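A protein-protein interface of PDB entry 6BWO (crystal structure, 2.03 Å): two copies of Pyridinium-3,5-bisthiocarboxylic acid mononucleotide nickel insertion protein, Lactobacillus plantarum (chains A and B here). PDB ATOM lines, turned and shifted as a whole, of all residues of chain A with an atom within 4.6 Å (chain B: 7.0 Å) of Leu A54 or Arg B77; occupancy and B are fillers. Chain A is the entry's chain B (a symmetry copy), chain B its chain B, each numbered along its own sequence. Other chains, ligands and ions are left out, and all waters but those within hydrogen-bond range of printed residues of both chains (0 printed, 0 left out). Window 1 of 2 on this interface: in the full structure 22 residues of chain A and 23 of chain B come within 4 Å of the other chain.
The side-chain amide nitrogen of Asn B11 sits at hydrogen-bond distance from the side-chain carboxylate of Asp A34 (2.9 Å). N of Tyr B78 lies within hydrogen-bond range of O of Gln A82, at 2.7 Å.
The side-chain carboxylate (OE2) of Glu B9 is in salt-bridge range of the side-chain amino group (NZ) of Lys B50, at 2.9 Å. NH2 of Arg B77 is in salt-bridge range of OE1 of Glu B9, at 2.6 Å. OD1 of Asn B11 sits at hydrogen-bond distance from NH2 of Arg B77. N of Trp A81 is in hydrogen-bond range of O of Val A5 (2.7 Å). The backbone NH (N) of Tyr A33 sits at hydrogen-bond distance from the backbone carbonyl oxygen (O) of Leu A54, 2.9 Å away. The backbone NH of Leu A54 lies within hydrogen-bond range of the backbone carbonyl oxygen of Asp A34, 2.8 Å away.
Met A7 touches Glu B9. CE of Met A7 touches NE of Arg B77, 3.4 Å away. Asn B11 touches Phe A36. Phe A36 touches Ile B40 (CD2 to CG2, 3.8 Å). Arg B77 touches Leu A54. Trp A81 touches Met B7 (CH2 to SD, 3.5 Å). Trp A81 touches Glu B9. Trp A81 touches Arg B77. Tyr B78 touches Trp A81 (C to CE3, 3.5 Å). N of Gln A82 touches NE2 of Gln B79 (3.95 Å).
Printed residues of chain B within 4 Å of Met A7: Glu B9 (3.7 Å) and Arg B77 (3.4 Å). Tyr A33 touches none of the printed residues of chain B. Printed residues of chain B within 4 Å of Asp A34: Asn B11 (2.9 Å). Of the printed residues of chain B, Arg A83 touches Val B76 (3.2 Å) and Tyr B78 (3.8 Å). Of chain A, only Met A7 (3.4 Å), Phe A36 (3.9 Å), Leu A54 (3.6 Å), Trp A81 (3.8 Å) and Gln A82 (3.1 Å) come within 4 Å of Arg B77. Of the printed residues of chain A, Gln B79 touches Trp A81 and Gln A82.
Of the 14 printed residues of chain A, 7 touch a printed residue of chain B. Hydrophobic or aromatic side chains of chain A within 4 Å of the printed part of chain B: Met A7, Phe A36, Leu A54 and Trp A81. Of the 15 printed residues of chain B, 8 touch a printed residue of chain A. Among the printed residues, 17 pairs touch across the chains. Among the printed residues, no Asp or Glu carboxylate lies within 4 Å of a Lys or Arg side-chain nitrogen of the other chain.
3 positions are printed for both chains. Of the 17 pairs that touch across the chains among the printed residues, none has its exchanged pair printed and touching as well.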
ATOM      1  N   VAL A   5     -27.212  16.647   6.316  1.00  0.00           N
ATOM      2  CA  VAL A   5     -26.438  17.533   7.173  1.00  0.00           C
ATOM      3  C   VAL A   5     -26.599  18.949   6.652  1.00  0.00           C
ATOM      4  O   VAL A   5     -26.662  19.176   5.440  1.00  0.00           O
ATOM      5  CB  VAL A   5     -24.951  17.110   7.226  1.00  0.00           C
ATOM      6  CG1 VAL A   5     -24.306  17.237   5.882  1.00  0.00           C
ATOM      7  CG2 VAL A   5     -24.192  17.918   8.229  1.00  0.00           C
ATOM      8  N   LEU A   6     -26.735  19.888   7.572  1.00  0.00           N
ATOM      9  CA  LEU A   6     -26.800  21.294   7.237  1.00  0.00           C
ATOM     10  C   LEU A   6     -25.381  21.824   7.192  1.00  0.00           C
ATOM     11  O   LEU A   6     -24.539  21.429   8.005  1.00  0.00           O
ATOM     12  CB  LEU A   6     -27.619  22.053   8.274  1.00  0.00           C
ATOM     13  CG  LEU A   6     -27.776  23.557   8.100  1.00  0.00           C
ATOM     14  CD1 LEU A   6     -28.899  23.823   7.147  1.00  0.00           C
ATOM     15  CD2 LEU A   6     -28.076  24.193   9.432  1.00  0.00           C
ATOM     16  N   MET A   7     -25.097  22.674   6.217  1.00  0.00           N
ATOM     17  CA  MET A   7     -23.822  23.369   6.168  1.00  0.00           C
ATOM     18  C   MET A   7     -24.079  24.857   6.287  1.00  0.00           C
ATOM     19  O   MET A   7     -24.851  25.411   5.505  1.00  0.00           O
ATOM     20  CB  MET A   7     -23.057  23.078   4.885  1.00  0.00           C
ATOM     21  CG  MET A   7     -21.857  23.966   4.715  1.00  0.00           C
ATOM     22  SD  MET A   7     -20.978  23.637   3.200  1.00  0.00           S
ATOM     23  CE  MET A   7     -20.572  21.921   3.406  1.00  0.00           C
ATOM     24  N   ALA A  32     -21.922  20.830  17.230  1.00  0.00           N
ATOM     25  CA  ALA A  32     -21.659  20.818  15.806  1.00  0.00           C
ATOM     26  C   ALA A  32     -20.942  19.530  15.446  1.00  0.00           C
ATOM     27  O   ALA A  32     -20.081  19.062  16.191  1.00  0.00           O
ATOM     28  CB  ALA A  32     -20.811  22.027  15.418  1.00  0.00           C
ATOM     29  N   TYR A  33     -21.330  18.929  14.316  1.00  0.00           N
ATOM     30  CA  TYR A  33     -20.645  17.724  13.855  1.00  0.00           C
ATOM     31  C   TYR A  33     -19.190  18.015  13.540  1.00  0.00           C
ATOM     32  O   TYR A  33     -18.300  17.217  13.857  1.00  0.00           O
ATOM     33  CB  TYR A  33     -21.293  17.145  12.595  1.00  0.00           C
ATOM     34  CG  TYR A  33     -22.704  16.674  12.720  1.00  0.00           C
ATOM     35  CD1 TYR A  33     -23.367  16.711  13.925  1.00  0.00           C
ATOM     36  CD2 TYR A  33     -23.367  16.166  11.625  1.00  0.00           C
ATOM     37  CE1 TYR A  33     -24.674  16.281  14.031  1.00  0.00           C
ATOM     38  CE2 TYR A  33     -24.668  15.730  11.721  1.00  0.00           C
ATOM     39  CZ  TYR A  33     -25.314  15.788  12.932  1.00  0.00           C
ATOM     40  OH  TYR A  33     -26.608  15.355  13.046  1.00  0.00           O
ATOM     41  N   ASP A  34     -18.937  19.144  12.883  1.00  0.00           N
ATOM     42  CA  ASP A  34     -17.604  19.519  12.450  1.00  0.00           C
ATOM     43  C   ASP A  34     -17.612  21.013  12.220  1.00  0.00           C
ATOM     44  O   ASP A  34     -18.654  21.605  11.954  1.00  0.00           O
ATOM     45  CB  ASP A  34     -17.199  18.774  11.170  1.00  0.00           C
ATOM     46  CG  ASP A  34     -15.699  18.610  11.031  1.00  0.00           C
ATOM     47  OD1 ASP A  34     -14.985  18.920  12.009  1.00  0.00           O
ATOM     48  OD2 ASP A  34     -15.243  18.159   9.945  1.00  0.00           O
ATOM     49  N   PHE A  36     -14.702  24.028  10.552  1.00  0.00           N
ATOM     50  CA  PHE A  36     -13.369  24.195  10.000  1.00  0.00           C
ATOM     51  C   PHE A  36     -13.183  25.586   9.420  1.00  0.00           C
ATOM     52  O   PHE A  36     -14.141  26.331   9.193  1.00  0.00           O
ATOM     53  CB  PHE A  36     -13.050  23.098   8.971  1.00  0.00           C
ATOM     54  CG  PHE A  36     -14.007  23.016   7.803  1.00  0.00           C
ATOM     55  CD1 PHE A  36     -15.202  22.331   7.917  1.00  0.00           C
ATOM     56  CD2 PHE A  36     -13.667  23.558   6.575  1.00  0.00           C
ATOM     57  CE1 PHE A  36     -16.053  22.217   6.850  1.00  0.00           C
ATOM     58  CE2 PHE A  36     -14.515  23.455   5.503  1.00  0.00           C
ATOM     59  CZ  PHE A  36     -15.708  22.776   5.636  1.00  0.00           C
ATOM     60  N   THR A  52     -16.852  27.382   8.378  1.00  0.00           N
ATOM     61  CA  THR A  52     -17.835  26.395   7.984  1.00  0.00           C
ATOM     62  C   THR A  52     -18.207  25.526   9.177  1.00  0.00           C
ATOM     63  O   THR A  52     -17.337  25.050   9.910  1.00  0.00           O
ATOM     64  CB  THR A  52     -17.316  25.531   6.851  1.00  0.00           C
ATOM     65  OG1 THR A  52     -16.879  26.372   5.780  1.00  0.00           O
ATOM     66  CG2 THR A  52     -18.431  24.643   6.359  1.00  0.00           C
ATOM     67  N   VAL A  53     -19.503  25.334   9.368  1.00  0.00           N
ATOM     68  CA  VAL A  53     -20.038  24.474  10.409  1.00  0.00           C
ATOM     69  C   VAL A  53     -20.915  23.421   9.758  1.00  0.00           C
ATOM     70  O   VAL A  53     -21.766  23.739   8.924  1.00  0.00           O
ATOM     71  CB  VAL A  53     -20.842  25.273  11.446  1.00  0.00           C
ATOM     72  CG1 VAL A  53     -21.322  24.357  12.556  1.00  0.00           C
ATOM     73  CG2 VAL A  53     -19.992  26.373  12.005  1.00  0.00           C
ATOM     74  N   LEU A  54     -20.709  22.172  10.139  1.00  0.00           N
ATOM     75  CA  LEU A  54     -21.606  21.100   9.760  1.00  0.00           C
ATOM     76  C   LEU A  54     -22.430  20.727  10.976  1.00  0.00           C
ATOM     77  O   LEU A  54     -21.908  20.678  12.090  1.00  0.00           O
ATOM     78  CB  LEU A  54     -20.831  19.893   9.259  1.00  0.00           C
ATOM     79  CG  LEU A  54     -20.058  20.179   7.978  1.00  0.00           C
ATOM     80  CD1 LEU A  54     -19.020  19.108   7.764  1.00  0.00           C
ATOM     81  CD2 LEU A  54     -21.003  20.252   6.794  1.00  0.00           C
ATOM     82  N   GLY A  55     -23.716  20.478  10.772  1.00  0.00           N
ATOM     83  CA  GLY A  55     -24.501  20.162  11.943  1.00  0.00           C
ATOM     84  C   GLY A  55     -25.804  19.481  11.606  1.00  0.00           C
ATOM     85  O   GLY A  55     -26.171  19.318  10.446  1.00  0.00           O
ATOM     86  N   TRP A  81     -26.924  19.263   2.742  1.00  0.00           N
ATOM     87  CA  TRP A  81     -26.235  18.327   1.872  1.00  0.00           C
ATOM     88  C   TRP A  81     -26.680  16.922   2.224  1.00  0.00           C
ATOM     89  O   TRP A  81     -27.097  16.661   3.347  1.00  0.00           O
ATOM     90  CB  TRP A  81     -24.711  18.431   2.005  1.00  0.00           C
ATOM     91  CG  TRP A  81     -24.111  19.695   1.476  1.00  0.00           C
ATOM     92  CD1 TRP A  81     -24.465  20.961   1.796  1.00  0.00           C
ATOM     93  CD2 TRP A  81     -23.022  19.807   0.556  1.00  0.00           C
ATOM     94  NE1 TRP A  81     -23.680  21.859   1.124  1.00  0.00           N
ATOM     95  CE2 TRP A  81     -22.780  21.168   0.361  1.00  0.00           C
ATOM     96  CE3 TRP A  81     -22.233  18.881  -0.122  1.00  0.00           C
ATOM     97  CZ2 TRP A  81     -21.785  21.629  -0.486  1.00  0.00           C
ATOM     98  CZ3 TRP A  81     -21.246  19.333  -0.952  1.00  0.00           C
ATOM     99  CH2 TRP A  81     -21.030  20.695  -1.137  1.00  0.00           C
ATOM    100  N   GLN A  82     -26.626  16.027   1.248  1.00  0.00           N
ATOM    101  CA  GLN A  82     -26.849  14.620   1.523  1.00  0.00           C
ATOM    102  C   GLN A  82     -25.546  13.957   1.940  1.00  0.00           C
ATOM    103  O   GLN A  82     -24.461  14.409   1.593  1.00  0.00           O
ATOM    104  CB  GLN A  82     -27.446  13.908   0.311  1.00  0.00           C
ATOM    105  CG  GLN A  82     -28.759  14.493  -0.092  1.00  0.00           C
ATOM    106  CD  GLN A  82     -29.733  14.453   1.053  1.00  0.00           C
ATOM    107  OE1 GLN A  82     -29.893  13.418   1.699  1.00  0.00           O
ATOM    108  NE2 GLN A  82     -30.366  15.591   1.343  1.00  0.00           N
ATOM    109  N   ARG A  83     -25.675  12.859   2.676  1.00  0.00           N
ATOM    110  CA  ARG A  83     -24.546  12.140   3.242  1.00  0.00           C
ATOM    111  C   ARG A  83     -24.589  10.666   2.869  1.00  0.00           C
ATOM    112  O   ARG A  83     -25.651  10.096   2.623  1.00  0.00           O
ATOM    113  CB  ARG A  83     -24.523  12.257   4.756  1.00  0.00           C
ATOM    114  CG  ARG A  83     -23.757  13.436   5.286  1.00  0.00           C
ATOM    115  CD  ARG A  83     -23.280  13.152   6.698  1.00  0.00           C
ATOM    116  NE  ARG A  83     -24.404  13.034   7.612  1.00  0.00           N
ATOM    117  CZ  ARG A  83     -24.286  12.963   8.931  1.00  0.00           C
ATOM    118  NH1 ARG A  83     -23.090  12.982   9.497  1.00  0.00           N
ATOM    119  NH2 ARG A  83     -25.371  12.874   9.682  1.00  0.00           N
ATOM    120  N   LEU B   6     -22.607  16.742  -9.708  1.00  0.00           N
ATOM    121  CA  LEU B   6     -22.601  16.368  -8.310  1.00  0.00           C
ATOM    122  C   LEU B   6     -21.300  16.858  -7.707  1.00  0.00           C
ATOM    123  O   LEU B   6     -20.251  16.809  -8.356  1.00  0.00           O
ATOM    124  CB  LEU B   6     -22.720  14.856  -8.162  1.00  0.00           C
ATOM    125  CG  LEU B   6     -22.705  14.272  -6.756  1.00  0.00           C
ATOM    126  CD1 LEU B   6     -24.085  14.350  -6.181  1.00  0.00           C
ATOM    127  CD2 LEU B   6     -22.254  12.836  -6.808  1.00  0.00           C
ATOM    128  N   MET B   7     -21.372  17.379  -6.491  1.00  0.00           N
ATOM    129  CA  MET B   7     -20.173  17.733  -5.749  1.00  0.00           C
ATOM    130  C   MET B   7     -20.113  16.883  -4.497  1.00  0.00           C
ATOM    131  O   MET B   7     -21.063  16.875  -3.715  1.00  0.00           O
ATOM    132  CB  MET B   7     -20.142  19.208  -5.375  1.00  0.00           C
ATOM    133  CG  MET B   7     -19.035  19.536  -4.414  1.00  0.00           C
ATOM    134  SD  MET B   7     -19.019  21.260  -3.960  1.00  0.00           S
ATOM    135  CE  MET B   7     -18.834  22.029  -5.550  1.00  0.00           C
ATOM    136  N   ILE B   8     -18.999  16.183  -4.308  1.00  0.00           N
ATOM    137  CA  ILE B   8     -18.761  15.342  -3.140  1.00  0.00           C
ATOM    138  C   ILE B   8     -17.624  15.960  -2.344  1.00  0.00           C
ATOM    139  O   ILE B   8     -16.621  16.381  -2.924  1.00  0.00           O
ATOM    140  CB  ILE B   8     -18.402  13.906  -3.553  1.00  0.00           C
ATOM    141  CG1 ILE B   8     -19.433  13.339  -4.507  1.00  0.00           C
ATOM    142  CG2 ILE B   8     -18.282  13.016  -2.355  1.00  0.00           C
ATOM    143  CD1 ILE B   8     -19.136  11.910  -4.866  1.00  0.00           C
ATOM    144  N   GLU B   9     -17.778  16.035  -1.023  1.00  0.00           N
ATOM    145  CA  GLU B   9     -16.755  16.634  -0.177  1.00  0.00           C
ATOM    146  C   GLU B   9     -16.360  15.708   0.961  1.00  0.00           C
ATOM    147  O   GLU B   9     -17.141  14.869   1.418  1.00  0.00           O
ATOM    148  CB  GLU B   9     -17.200  17.950   0.448  1.00  0.00           C
ATOM    149  CG  GLU B   9     -17.289  19.101  -0.491  1.00  0.00           C
ATOM    150  CD  GLU B   9     -17.407  20.412   0.245  1.00  0.00           C
ATOM    151  OE1 GLU B   9     -17.867  20.421   1.402  1.00  0.00           O
ATOM    152  OE2 GLU B   9     -17.041  21.445  -0.340  1.00  0.00           O
ATOM    153  N   ALA B  10     -15.141  15.909   1.450  1.00  0.00           N
ATOM    154  CA  ALA B  10     -14.676  15.168   2.610  1.00  0.00           C
ATOM    155  C   ALA B  10     -13.575  15.950   3.310  1.00  0.00           C
ATOM    156  O   ALA B  10     -12.702  16.517   2.655  1.00  0.00           O
ATOM    157  CB  ALA B  10     -14.181  13.775   2.211  1.00  0.00           C
ATOM    158  N   ASN B  11     -13.649  15.981   4.641  1.00  0.00           N
ATOM    159  CA  ASN B  11     -12.667  16.605   5.517  1.00  0.00           C
ATOM    160  C   ASN B  11     -11.751  15.546   6.091  1.00  0.00           C
ATOM    161  O   ASN B  11     -12.218  14.621   6.755  1.00  0.00           O
ATOM    162  CB  ASN B  11     -13.325  17.310   6.701  1.00  0.00           C
ATOM    163  CG  ASN B  11     -14.107  18.497   6.311  1.00  0.00           C
ATOM    164  OD1 ASN B  11     -14.177  18.852   5.147  1.00  0.00           O
ATOM    165  ND2 ASN B  11     -14.718  19.126   7.292  1.00  0.00           N
ATOM    166  N   ILE B  40      -7.546  23.329   4.898  1.00  0.00           N
ATOM    167  CA  ILE B  40      -8.488  23.700   5.947  1.00  0.00           C
ATOM    168  C   ILE B  40      -7.874  23.405   7.306  1.00  0.00           C
ATOM    169  O   ILE B  40      -6.952  22.607   7.441  1.00  0.00           O
ATOM    170  CB  ILE B  40      -9.843  22.970   5.798  1.00  0.00           C
ATOM    171  CG1 ILE B  40      -9.663  21.465   5.971  1.00  0.00           C
ATOM    172  CG2 ILE B  40     -10.500  23.281   4.463  1.00  0.00           C
ATOM    173  CD1 ILE B  40     -10.977  20.718   6.118  1.00  0.00           C
ATOM    174  N   LYS B  50      -9.457  19.510   2.679  1.00  0.00           N
ATOM    175  CA  LYS B  50     -10.760  19.115   2.168  1.00  0.00           C
ATOM    176  C   LYS B  50     -10.600  18.559   0.762  1.00  0.00           C
ATOM    177  O   LYS B  50      -9.971  19.183  -0.095  1.00  0.00           O
ATOM    178  CB  LYS B  50     -11.755  20.270   2.158  1.00  0.00           C
ATOM    179  CG  LYS B  50     -13.191  19.821   1.849  1.00  0.00           C
ATOM    180  CD  LYS B  50     -14.135  20.994   1.857  1.00  0.00           C
ATOM    181  CE  LYS B  50     -13.948  21.827   0.607  1.00  0.00           C
ATOM    182  NZ  LYS B  50     -14.785  23.053   0.598  1.00  0.00           N
ATOM    183  N   LEU B  51     -11.162  17.386   0.535  1.00  0.00           N
ATOM    184  CA  LEU B  51     -11.150  16.762  -0.777  1.00  0.00           C
ATOM    185  C   LEU B  51     -12.487  17.014  -1.464  1.00  0.00           C
ATOM    186  O   LEU B  51     -13.534  16.578  -0.975  1.00  0.00           O
ATOM    187  CB  LEU B  51     -10.882  15.264  -0.658  1.00  0.00           C
ATOM    188  CG  LEU B  51     -11.196  14.449  -1.913  1.00  0.00           C
ATOM    189  CD1 LEU B  51     -10.077  14.626  -2.923  1.00  0.00           C
ATOM    190  CD2 LEU B  51     -11.325  12.994  -1.571  1.00  0.00           C
ATOM    191  N   THR B  52     -12.445  17.679  -2.612  1.00  0.00           N
ATOM    192  CA  THR B  52     -13.638  17.929  -3.393  1.00  0.00           C
ATOM    193  C   THR B  52     -13.546  17.207  -4.730  1.00  0.00           C
ATOM    194  O   THR B  52     -12.521  17.267  -5.414  1.00  0.00           O
ATOM    195  CB  THR B  52     -13.841  19.416  -3.616  1.00  0.00           C
ATOM    196  OG1 THR B  52     -13.825  20.087  -2.354  1.00  0.00           O
ATOM    197  CG2 THR B  52     -15.180  19.634  -4.275  1.00  0.00           C
ATOM    198  N   GLY B  75     -17.667   9.366   6.453  1.00  0.00           N
ATOM    199  CA  GLY B  75     -18.799   9.739   5.634  1.00  0.00           C
ATOM    200  C   GLY B  75     -18.359  10.754   4.604  1.00  0.00           C
ATOM    201  O   GLY B  75     -17.283  11.342   4.699  1.00  0.00           O
ATOM    202  N   VAL B  76     -19.184  10.912   3.586  1.00  0.00           N
ATOM    203  CA  VAL B  76     -18.995  11.967   2.607  1.00  0.00           C
ATOM    204  C   VAL B  76     -20.296  12.743   2.551  1.00  0.00           C
ATOM    205  O   VAL B  76     -21.348  12.261   2.965  1.00  0.00           O
ATOM    206  CB  VAL B  76     -18.629  11.426   1.213  1.00  0.00           C
ATOM    207  CG1 VAL B  76     -17.413  10.547   1.293  1.00  0.00           C
ATOM    208  CG2 VAL B  76     -19.791  10.672   0.619  1.00  0.00           C
ATOM    209  N   ARG B  77     -20.218  13.952   2.026  1.00  0.00           N
ATOM    210  CA  ARG B  77     -21.396  14.765   1.787  1.00  0.00           C
ATOM    211  C   ARG B  77     -21.432  15.142   0.316  1.00  0.00           C
ATOM    212  O   ARG B  77     -20.392  15.324  -0.319  1.00  0.00           O
ATOM    213  CB  ARG B  77     -21.398  16.026   2.640  1.00  0.00           C
ATOM    214  CG  ARG B  77     -20.132  16.852   2.514  1.00  0.00           C
ATOM    215  CD  ARG B  77     -20.188  18.036   3.431  1.00  0.00           C
ATOM    216  NE  ARG B  77     -19.053  18.923   3.273  1.00  0.00           N
ATOM    217  CZ  ARG B  77     -17.897  18.769   3.900  1.00  0.00           C
ATOM    218  NH1 ARG B  77     -17.716  17.744   4.717  1.00  0.00           N
ATOM    219  NH2 ARG B  77     -16.920  19.647   3.708  1.00  0.00           N
ATOM    220  N   TYR B  78     -22.630  15.231  -0.240  1.00  0.00           N
ATOM    221  CA  TYR B  78     -22.709  15.542  -1.647  1.00  0.00           C
ATOM    222  C   TYR B  78     -23.911  16.423  -1.903  1.00  0.00           C
ATOM    223  O   TYR B  78     -24.887  16.427  -1.148  1.00  0.00           O
ATOM    224  CB  TYR B  78     -22.764  14.301  -2.518  1.00  0.00           C
ATOM    225  CG  TYR B  78     -23.833  13.316  -2.164  1.00  0.00           C
ATOM    226  CD1 TYR B  78     -25.038  13.316  -2.846  1.00  0.00           C
ATOM    227  CD2 TYR B  78     -23.644  12.375  -1.175  1.00  0.00           C
ATOM    228  CE1 TYR B  78     -26.029  12.424  -2.547  1.00  0.00           C
ATOM    229  CE2 TYR B  78     -24.633  11.467  -0.874  1.00  0.00           C
ATOM    230  CZ  TYR B  78     -25.820  11.501  -1.568  1.00  0.00           C
ATOM    231  OH  TYR B  78     -26.811  10.613  -1.287  1.00  0.00           O
ATOM    232  N   GLN B  79     -23.807  17.175  -2.984  1.00  0.00           N
ATOM    233  CA  GLN B  79     -24.827  18.109  -3.399  1.00  0.00           C
ATOM    234  C   GLN B  79     -24.760  18.166  -4.913  1.00  0.00           C
ATOM    235  O   GLN B  79     -23.713  17.907  -5.508  1.00  0.00           O
ATOM    236  CB  GLN B  79     -24.566  19.482  -2.751  1.00  0.00           C
ATOM    237  CG  GLN B  79     -25.741  20.431  -2.580  1.00  0.00           C
ATOM    238  CD  GLN B  79     -27.067  19.737  -2.351  1.00  0.00           C
ATOM    239  OE1 GLN B  79     -27.960  19.815  -3.187  1.00  0.00           O
ATOM    240  NE2 GLN B  79     -27.203  19.055  -1.224  1.00  0.00           N
